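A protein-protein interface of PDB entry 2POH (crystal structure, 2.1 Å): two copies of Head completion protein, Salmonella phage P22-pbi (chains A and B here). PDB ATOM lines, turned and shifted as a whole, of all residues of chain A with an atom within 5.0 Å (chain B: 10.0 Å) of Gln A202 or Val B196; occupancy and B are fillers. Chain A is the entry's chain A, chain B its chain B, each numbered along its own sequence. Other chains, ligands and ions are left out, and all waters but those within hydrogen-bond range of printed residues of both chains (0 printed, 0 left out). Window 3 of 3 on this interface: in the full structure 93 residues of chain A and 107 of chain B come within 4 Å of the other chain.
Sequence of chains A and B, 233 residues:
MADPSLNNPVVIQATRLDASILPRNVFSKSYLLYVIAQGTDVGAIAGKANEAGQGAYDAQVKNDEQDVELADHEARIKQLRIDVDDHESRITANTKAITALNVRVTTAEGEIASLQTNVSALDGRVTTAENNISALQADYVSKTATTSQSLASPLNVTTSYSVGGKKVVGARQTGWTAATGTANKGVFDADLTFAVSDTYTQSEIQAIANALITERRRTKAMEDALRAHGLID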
ATOM      1  N   TYR A 200     -22.678 -13.230 -10.892  1.00  0.00           N
ATOM      2  CA  TYR A 200     -23.217 -14.495 -11.332  1.00  0.00           C
ATOM      3  C   TYR A 200     -23.336 -14.723 -12.825  1.00  0.00           C
ATOM      4  O   TYR A 200     -22.349 -15.151 -13.428  1.00  0.00           O
ATOM      5  CB  TYR A 200     -24.610 -14.568 -10.683  1.00  0.00           C
ATOM      6  CG  TYR A 200     -25.374 -15.833 -10.949  1.00  0.00           C
ATOM      7  CD1 TYR A 200     -24.963 -17.069 -10.452  1.00  0.00           C
ATOM      8  CD2 TYR A 200     -26.545 -15.770 -11.702  1.00  0.00           C
ATOM      9  CE1 TYR A 200     -25.704 -18.202 -10.718  1.00  0.00           C
ATOM     10  CE2 TYR A 200     -27.285 -16.908 -11.967  1.00  0.00           C
ATOM     11  CZ  TYR A 200     -26.854 -18.120 -11.471  1.00  0.00           C
ATOM     12  OH  TYR A 200     -27.568 -19.268 -11.718  1.00  0.00           O
ATOM     13  N   THR A 201     -24.473 -14.466 -13.458  1.00  0.00           N
ATOM     14  CA  THR A 201     -24.725 -14.741 -14.861  1.00  0.00           C
ATOM     15  C   THR A 201     -24.990 -16.230 -15.125  1.00  0.00           C
ATOM     16  O   THR A 201     -24.123 -17.106 -15.130  1.00  0.00           O
ATOM     17  CB  THR A 201     -23.598 -14.261 -15.801  1.00  0.00           C
ATOM     18  OG1 THR A 201     -23.124 -12.987 -15.353  1.00  0.00           O
ATOM     19  CG2 THR A 201     -24.120 -14.072 -17.217  1.00  0.00           C
ATOM     20  N   GLN A 202     -26.267 -16.493 -15.381  1.00  0.00           N
ATOM     21  CA  GLN A 202     -26.776 -17.815 -15.750  1.00  0.00           C
ATOM     22  C   GLN A 202     -26.188 -18.298 -17.076  1.00  0.00           C
ATOM     23  O   GLN A 202     -25.844 -19.475 -17.169  1.00  0.00           O
ATOM     24  CB  GLN A 202     -28.300 -17.859 -15.768  1.00  0.00           C
ATOM     25  CG  GLN A 202     -29.002 -18.325 -17.031  1.00  0.00           C
ATOM     26  CD  GLN A 202     -30.328 -19.006 -16.790  1.00  0.00           C
ATOM     27  OE1 GLN A 202     -31.373 -18.565 -17.273  1.00  0.00           O
ATOM     28  NE2 GLN A 202     -30.285 -20.097 -16.038  1.00  0.00           N
ATOM     29  N   SER A 203     -26.065 -17.443 -18.084  1.00  0.00           N
ATOM     30  CA  SER A 203     -25.540 -17.851 -19.372  1.00  0.00           C
ATOM     31  C   SER A 203     -24.145 -18.457 -19.264  1.00  0.00           C
ATOM     32  O   SER A 203     -23.783 -19.264 -20.113  1.00  0.00           O
ATOM     33  CB  SER A 203     -25.543 -16.660 -20.332  1.00  0.00           C
ATOM     34  OG  SER A 203     -24.265 -16.417 -20.874  1.00  0.00           O
ATOM     35  N   GLU A 204     -23.394 -18.061 -18.257  1.00  0.00           N
ATOM     36  CA  GLU A 204     -21.978 -18.433 -18.195  1.00  0.00           C
ATOM     37  C   GLU A 204     -21.816 -19.667 -17.342  1.00  0.00           C
ATOM     38  O   GLU A 204     -20.930 -20.498 -17.549  1.00  0.00           O
ATOM     39  CB  GLU A 204     -21.159 -17.251 -17.690  1.00  0.00           C
ATOM     40  CG  GLU A 204     -20.434 -16.414 -18.720  1.00  0.00           C
ATOM     41  CD  GLU A 204     -21.142 -15.119 -19.090  1.00  0.00           C
ATOM     42  OE1 GLU A 204     -22.057 -15.196 -19.937  1.00  0.00           O
ATOM     43  OE2 GLU A 204     -20.832 -14.032 -18.565  1.00  0.00           O
ATOM     44  N   ILE A 205     -22.699 -19.863 -16.371  1.00  0.00           N
ATOM     45  CA  ILE A 205     -22.730 -21.072 -15.537  1.00  0.00           C
ATOM     46  C   ILE A 205     -23.111 -22.224 -16.461  1.00  0.00           C
ATOM     47  O   ILE A 205     -22.539 -23.312 -16.385  1.00  0.00           O
ATOM     48  CB  ILE A 205     -23.644 -20.984 -14.315  1.00  0.00           C
ATOM     49  CG1 ILE A 205     -24.636 -22.130 -14.027  1.00  0.00           C
ATOM     50  CG2 ILE A 205     -24.535 -19.756 -14.326  1.00  0.00           C
ATOM     51  CD1 ILE A 205     -23.953 -23.348 -13.483  1.00  0.00           C
ATOM     52  N   GLN A 206     -24.066 -21.990 -17.336  1.00  0.00           N
ATOM     53  CA  GLN A 206     -24.563 -22.977 -18.274  1.00  0.00           C
ATOM     54  C   GLN A 206     -23.465 -23.454 -19.216  1.00  0.00           C
ATOM     55  O   GLN A 206     -23.406 -24.639 -19.556  1.00  0.00           O
ATOM     56  CB  GLN A 206     -25.714 -22.399 -19.101  1.00  0.00           C
ATOM     57  CG  GLN A 206     -26.862 -21.839 -18.272  1.00  0.00           C
ATOM     58  CD  GLN A 206     -27.932 -21.175 -19.111  1.00  0.00           C
ATOM     59  OE1 GLN A 206     -29.006 -21.732 -19.338  1.00  0.00           O
ATOM     60  NE2 GLN A 206     -27.646 -19.964 -19.580  1.00  0.00           N
ATOM     61  N   THR B 193     -28.417 -34.404 -17.585  1.00  0.00           N
ATOM     62  CA  THR B 193     -28.357 -32.965 -17.572  1.00  0.00           C
ATOM     63  C   THR B 193     -28.262 -32.495 -16.119  1.00  0.00           C
ATOM     64  O   THR B 193     -27.762 -33.224 -15.269  1.00  0.00           O
ATOM     65  CB  THR B 193     -29.560 -32.413 -18.332  1.00  0.00           C
ATOM     66  OG1 THR B 193     -30.756 -32.708 -17.601  1.00  0.00           O
ATOM     67  CG2 THR B 193     -29.637 -33.109 -19.726  1.00  0.00           C
ATOM     68  N   PHE B 194     -28.725 -31.285 -15.829  1.00  0.00           N
ATOM     69  CA  PHE B 194     -28.280 -30.590 -14.632  1.00  0.00           C
ATOM     70  C   PHE B 194     -29.304 -29.652 -13.997  1.00  0.00           C
ATOM     71  O   PHE B 194     -29.424 -29.678 -12.765  1.00  0.00           O
ATOM     72  CB  PHE B 194     -27.017 -29.762 -14.945  1.00  0.00           C
ATOM     73  CG  PHE B 194     -25.765 -30.559 -14.597  1.00  0.00           C
ATOM     74  CD1 PHE B 194     -24.798 -30.776 -15.562  1.00  0.00           C
ATOM     75  CD2 PHE B 194     -25.601 -31.069 -13.318  1.00  0.00           C
ATOM     76  CE1 PHE B 194     -23.662 -31.510 -15.266  1.00  0.00           C
ATOM     77  CE2 PHE B 194     -24.463 -31.805 -13.016  1.00  0.00           C
ATOM     78  CZ  PHE B 194     -23.509 -32.006 -13.989  1.00  0.00           C
ATOM     79  N   ALA B 195     -29.970 -28.860 -14.815  1.00  0.00           N
ATOM     80  CA  ALA B 195     -30.990 -27.893 -14.461  1.00  0.00           C
ATOM     81  C   ALA B 195     -30.454 -26.523 -14.042  1.00  0.00           C
ATOM     82  O   ALA B 195     -29.888 -26.397 -12.946  1.00  0.00           O
ATOM     83  CB  ALA B 195     -31.852 -28.402 -13.310  1.00  0.00           C
ATOM     84  N   VAL B 196     -30.689 -25.500 -14.844  1.00  0.00           N
ATOM     85  CA  VAL B 196     -30.251 -24.128 -14.576  1.00  0.00           C
ATOM     86  C   VAL B 196     -31.423 -23.154 -14.631  1.00  0.00           C
ATOM     87  O   VAL B 196     -32.194 -23.072 -15.584  1.00  0.00           O
ATOM     88  CB  VAL B 196     -29.117 -23.663 -15.513  1.00  0.00           C
ATOM     89  CG1 VAL B 196     -29.652 -22.938 -16.740  1.00  0.00           C
ATOM     90  CG2 VAL B 196     -28.147 -22.769 -14.749  1.00  0.00           C
ATOM     91  N   SER B 197     -31.561 -22.388 -13.547  1.00  0.00           N
ATOM     92  CA  SER B 197     -32.635 -21.421 -13.416  1.00  0.00           C
ATOM     93  C   SER B 197     -32.097 -19.991 -13.312  1.00  0.00           C
ATOM     94  O   SER B 197     -30.894 -19.777 -13.436  1.00  0.00           O
ATOM     95  CB  SER B 197     -33.502 -21.707 -12.186  1.00  0.00           C
ATOM     96  OG  SER B 197     -32.952 -22.748 -11.400  1.00  0.00           O
ATOM     97  N   ASP B 198     -33.031 -19.090 -13.085  1.00  0.00           N
ATOM     98  CA  ASP B 198     -32.889 -17.669 -12.892  1.00  0.00           C
ATOM     99  C   ASP B 198     -31.750 -17.314 -11.945  1.00  0.00           C
ATOM    100  O   ASP B 198     -30.650 -16.966 -12.368  1.00  0.00           O
ATOM    101  CB  ASP B 198     -34.192 -17.088 -12.319  1.00  0.00           C
ATOM    102  CG  ASP B 198     -35.205 -16.739 -13.393  1.00  0.00           C
ATOM    103  OD1 ASP B 198     -34.787 -16.531 -14.551  1.00  0.00           O
ATOM    104  OD2 ASP B 198     -36.415 -16.673 -13.079  1.00  0.00           O
ATOM    105  N   THR B 199     -32.042 -17.400 -10.649  1.00  0.00           N
ATOM    106  CA  THR B 199     -31.051 -17.029  -9.638  1.00  0.00           C
ATOM    107  C   THR B 199     -30.183 -18.223  -9.250  1.00  0.00           C
ATOM    108  O   THR B 199     -30.404 -19.345  -9.719  1.00  0.00           O
ATOM    109  CB  THR B 199     -31.750 -16.406  -8.418  1.00  0.00           C
ATOM    110  OG1 THR B 199     -30.773 -15.925  -7.482  1.00  0.00           O
ATOM    111  CG2 THR B 199     -32.606 -17.432  -7.686  1.00  0.00           C
ATOM    112  N   TYR B 200     -29.197 -17.971  -8.414  1.00  0.00           N
ATOM    113  CA  TYR B 200     -28.151 -18.856  -7.939  1.00  0.00           C
ATOM    114  C   TYR B 200     -28.581 -20.314  -7.834  1.00  0.00           C
ATOM    115  O   TYR B 200     -28.229 -21.138  -8.688  1.00  0.00           O
ATOM    116  CB  TYR B 200     -27.656 -18.366  -6.573  1.00  0.00           C
ATOM    117  CG  TYR B 200     -26.282 -18.819  -6.149  1.00  0.00           C
ATOM    118  CD1 TYR B 200     -25.127 -18.244  -6.663  1.00  0.00           C
ATOM    119  CD2 TYR B 200     -26.130 -19.837  -5.214  1.00  0.00           C
ATOM    120  CE1 TYR B 200     -23.880 -18.679  -6.258  1.00  0.00           C
ATOM    121  CE2 TYR B 200     -24.888 -20.277  -4.801  1.00  0.00           C
ATOM    122  CZ  TYR B 200     -23.759 -19.688  -5.329  1.00  0.00           C
ATOM    123  OH  TYR B 200     -22.515 -20.116  -4.926  1.00  0.00           O
ATOM    124  N   THR B 201     -29.319 -20.656  -6.786  1.00  0.00           N
ATOM    125  CA  THR B 201     -29.648 -22.056  -6.529  1.00  0.00           C
ATOM    126  C   THR B 201     -28.379 -22.879  -6.285  1.00  0.00           C
ATOM    127  O   THR B 201     -27.671 -23.312  -7.199  1.00  0.00           O
ATOM    128  CB  THR B 201     -30.455 -22.692  -7.673  1.00  0.00           C
ATOM    129  OG1 THR B 201     -31.283 -21.709  -8.305  1.00  0.00           O
ATOM    130  CG2 THR B 201     -31.372 -23.785  -7.136  1.00  0.00           C
ATOM    131  N   GLN B 202     -28.127 -23.085  -5.005  1.00  0.00           N
ATOM    132  CA  GLN B 202     -26.972 -23.780  -4.460  1.00  0.00           C
ATOM    133  C   GLN B 202     -26.958 -25.249  -4.856  1.00  0.00           C
ATOM    134  O   GLN B 202     -25.890 -25.796  -5.129  1.00  0.00           O
ATOM    135  CB  GLN B 202     -26.965 -23.609  -2.931  1.00  0.00           C
ATOM    136  CG  GLN B 202     -25.752 -24.188  -2.232  1.00  0.00           C
ATOM    137  CD  GLN B 202     -25.914 -24.366  -0.740  1.00  0.00           C
ATOM    138  OE1 GLN B 202     -24.918 -24.540  -0.028  1.00  0.00           O
ATOM    139  NE2 GLN B 202     -27.146 -24.326  -0.246  1.00  0.00           N
ATOM    140  N   SER B 203     -28.127 -25.881  -4.902  1.00  0.00           N
ATOM    141  CA  SER B 203     -28.259 -27.274  -5.312  1.00  0.00           C
ATOM    142  C   SER B 203     -28.012 -27.412  -6.810  1.00  0.00           C
ATOM    143  O   SER B 203     -27.532 -28.432  -7.309  1.00  0.00           O
ATOM    144  CB  SER B 203     -29.644 -27.819  -4.967  1.00  0.00           C
ATOM    145  OG  SER B 203     -30.586 -27.460  -5.965  1.00  0.00           O
ATOM    146  N   GLU B 204     -28.356 -26.348  -7.514  1.00  0.00           N
ATOM    147  CA  GLU B 204     -28.139 -26.203  -8.944  1.00  0.00           C
ATOM    148  C   GLU B 204     -26.644 -26.197  -9.240  1.00  0.00           C
ATOM    149  O   GLU B 204     -26.194 -26.578 -10.315  1.00  0.00           O
ATOM    150  CB  GLU B 204     -28.755 -24.904  -9.411  1.00  0.00           C
ATOM    151  CG  GLU B 204     -29.122 -24.714 -10.858  1.00  0.00           C
ATOM    152  CD  GLU B 204     -29.974 -23.466 -11.044  1.00  0.00           C
ATOM    153  OE1 GLU B 204     -31.000 -23.343 -10.341  1.00  0.00           O
ATOM    154  OE2 GLU B 204     -29.599 -22.620 -11.880  1.00  0.00           O
ATOM    155  N   ILE B 205     -25.893 -25.744  -8.238  1.00  0.00           N
ATOM    156  CA  ILE B 205     -24.443 -25.642  -8.414  1.00  0.00           C
ATOM    157  C   ILE B 205     -23.726 -26.875  -7.883  1.00  0.00           C
ATOM    158  O   ILE B 205     -22.849 -27.422  -8.563  1.00  0.00           O
ATOM    159  CB  ILE B 205     -23.956 -24.337  -7.758  1.00  0.00           C
ATOM    160  CG1 ILE B 205     -23.535 -23.315  -8.828  1.00  0.00           C
ATOM    161  CG2 ILE B 205     -22.862 -24.530  -6.735  1.00  0.00           C
ATOM    162  CD1 ILE B 205     -24.255 -23.552 -10.144  1.00  0.00           C
ATOM    163  N   ALA B 207     -24.687 -29.763  -7.739  1.00  0.00           N
ATOM    164  CA  ALA B 207     -24.916 -30.833  -8.702  1.00  0.00           C
ATOM    165  C   ALA B 207     -23.790 -30.945  -9.724  1.00  0.00           C
ATOM    166  O   ALA B 207     -23.322 -32.051  -9.998  1.00  0.00           O
ATOM    167  CB  ALA B 207     -26.248 -30.625  -9.413  1.00  0.00           C
ATOM    168  N   ILE B 208     -23.359 -29.818 -10.291  1.00  0.00           N
ATOM    169  CA  ILE B 208     -22.369 -29.857 -11.370  1.00  0.00           C
ATOM    170  C   ILE B 208     -20.955 -30.077 -10.851  1.00  0.00           C
ATOM    171  O   ILE B 208     -20.157 -30.785 -11.467  1.00  0.00           O
ATOM    172  CB  ILE B 208     -22.440 -28.578 -12.228  1.00  0.00           C
ATOM    173  CG1 ILE B 208     -21.742 -27.344 -11.657  1.00  0.00           C
ATOM    174  CG2 ILE B 208     -23.901 -28.254 -12.540  1.00  0.00           C
ATOM    175  CD1 ILE B 208     -22.457 -26.055 -12.025  1.00  0.00           C
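O of Gln A202 lies close to NE2 of Gln A206, 3.0 Å away. The backbone NH of Ser A203 lies close to the side-chain amide nitrogen of Gln A206 (3.3 Å). The side-chain carboxylate (OE2) of Glu B204 sits at hydrogen-bond distance from the backbone NH (N) of Ser B197, 2.6 Å away. The backbone carbonyl oxygen (O) of Thr B199 lies within hydrogen-bond range of the side-chain hydroxyl (OG1) of Thr B201, at 2.9 Å. The side-chain hydroxyl (OG1) of Thr B201 sits at hydrogen-bond distance from the side-chain carboxylate (OE1) of Glu B204 (2.6 Å).
Tyr B200 touches its own counterpart, Tyr A200. Tyr A200 touches Glu B204, but with the chains exchanged Glu A204 does not touch Tyr B200 (10.9 Å). Ile B205 touches its own counterpart, Ile A205. Positions printed for both chains: 200, 201, 202, 203, 204 and 205.
Of the 15 printed residues of chain B, 8 touch a printed residue of chain A. Along chain B the printed residues that touch a printed residue of chain A span positions 196 to 208. Hydrophobic or aromatic side chains of chain A that line the printed part of chain B: Tyr A200 and Ile A205. Among the printed residues, 11 pairs touch across the chains.
Ser B197 touches Tyr A200. Tyr A200 touches Asp B198 (CE2 to O, 3.4 Å). Tyr A200 touches Tyr B200 (OH to O, 3.6 Å). Glu B204 touches Tyr A200 (OE2 to OH, 3.9 Å). NE2 of Gln A202 touches CG1 of Val B196 (3.0 Å). Ile A205 touches Val B196 (CG1 to CG2, 3.6 Å). CD1 of Ile A205 touches CD1 of Ile B205, 3.4 Å away. Ile A205 touches Ile B208. CG1 of Val B196 touches OE1 of Gln A206, 2.9 Å away.
Of chain B, only Val B196 (3.0 Å) and Ser B197 (2.7 Å) come within 4 Å of Gln A202. Val B196 touches three residues of chain A. Thr A201 touches none of the printed residues of chain B. No residue of chain B comes within 4 Å of Ser A203. Printed residues of chain A within 4 Å of Tyr B200: Tyr A200 (3.6 Å). Printed residues of chain A within 4 Å of Thr B199: Tyr A200 (3.5 Å). Printed residues of chain A within 4 Å of Ser B197: Tyr A200 (3.8 Å) and Gln A202 (2.7 Å). Ser B203 touches none of the printed residues of chain A. The nearest printed residue of chain A that does not touch Ile B205 is Tyr A200 (5.6 Å).
The side-chain hydroxyl (OH) of Tyr A200 lies within hydrogen-bond range of the backbone carbonyl oxygen (O) of Thr B199 (3.5 Å). NE2 of Gln A202 sits at hydrogen-bond distance from O of Ser B197 (2.7 Å).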
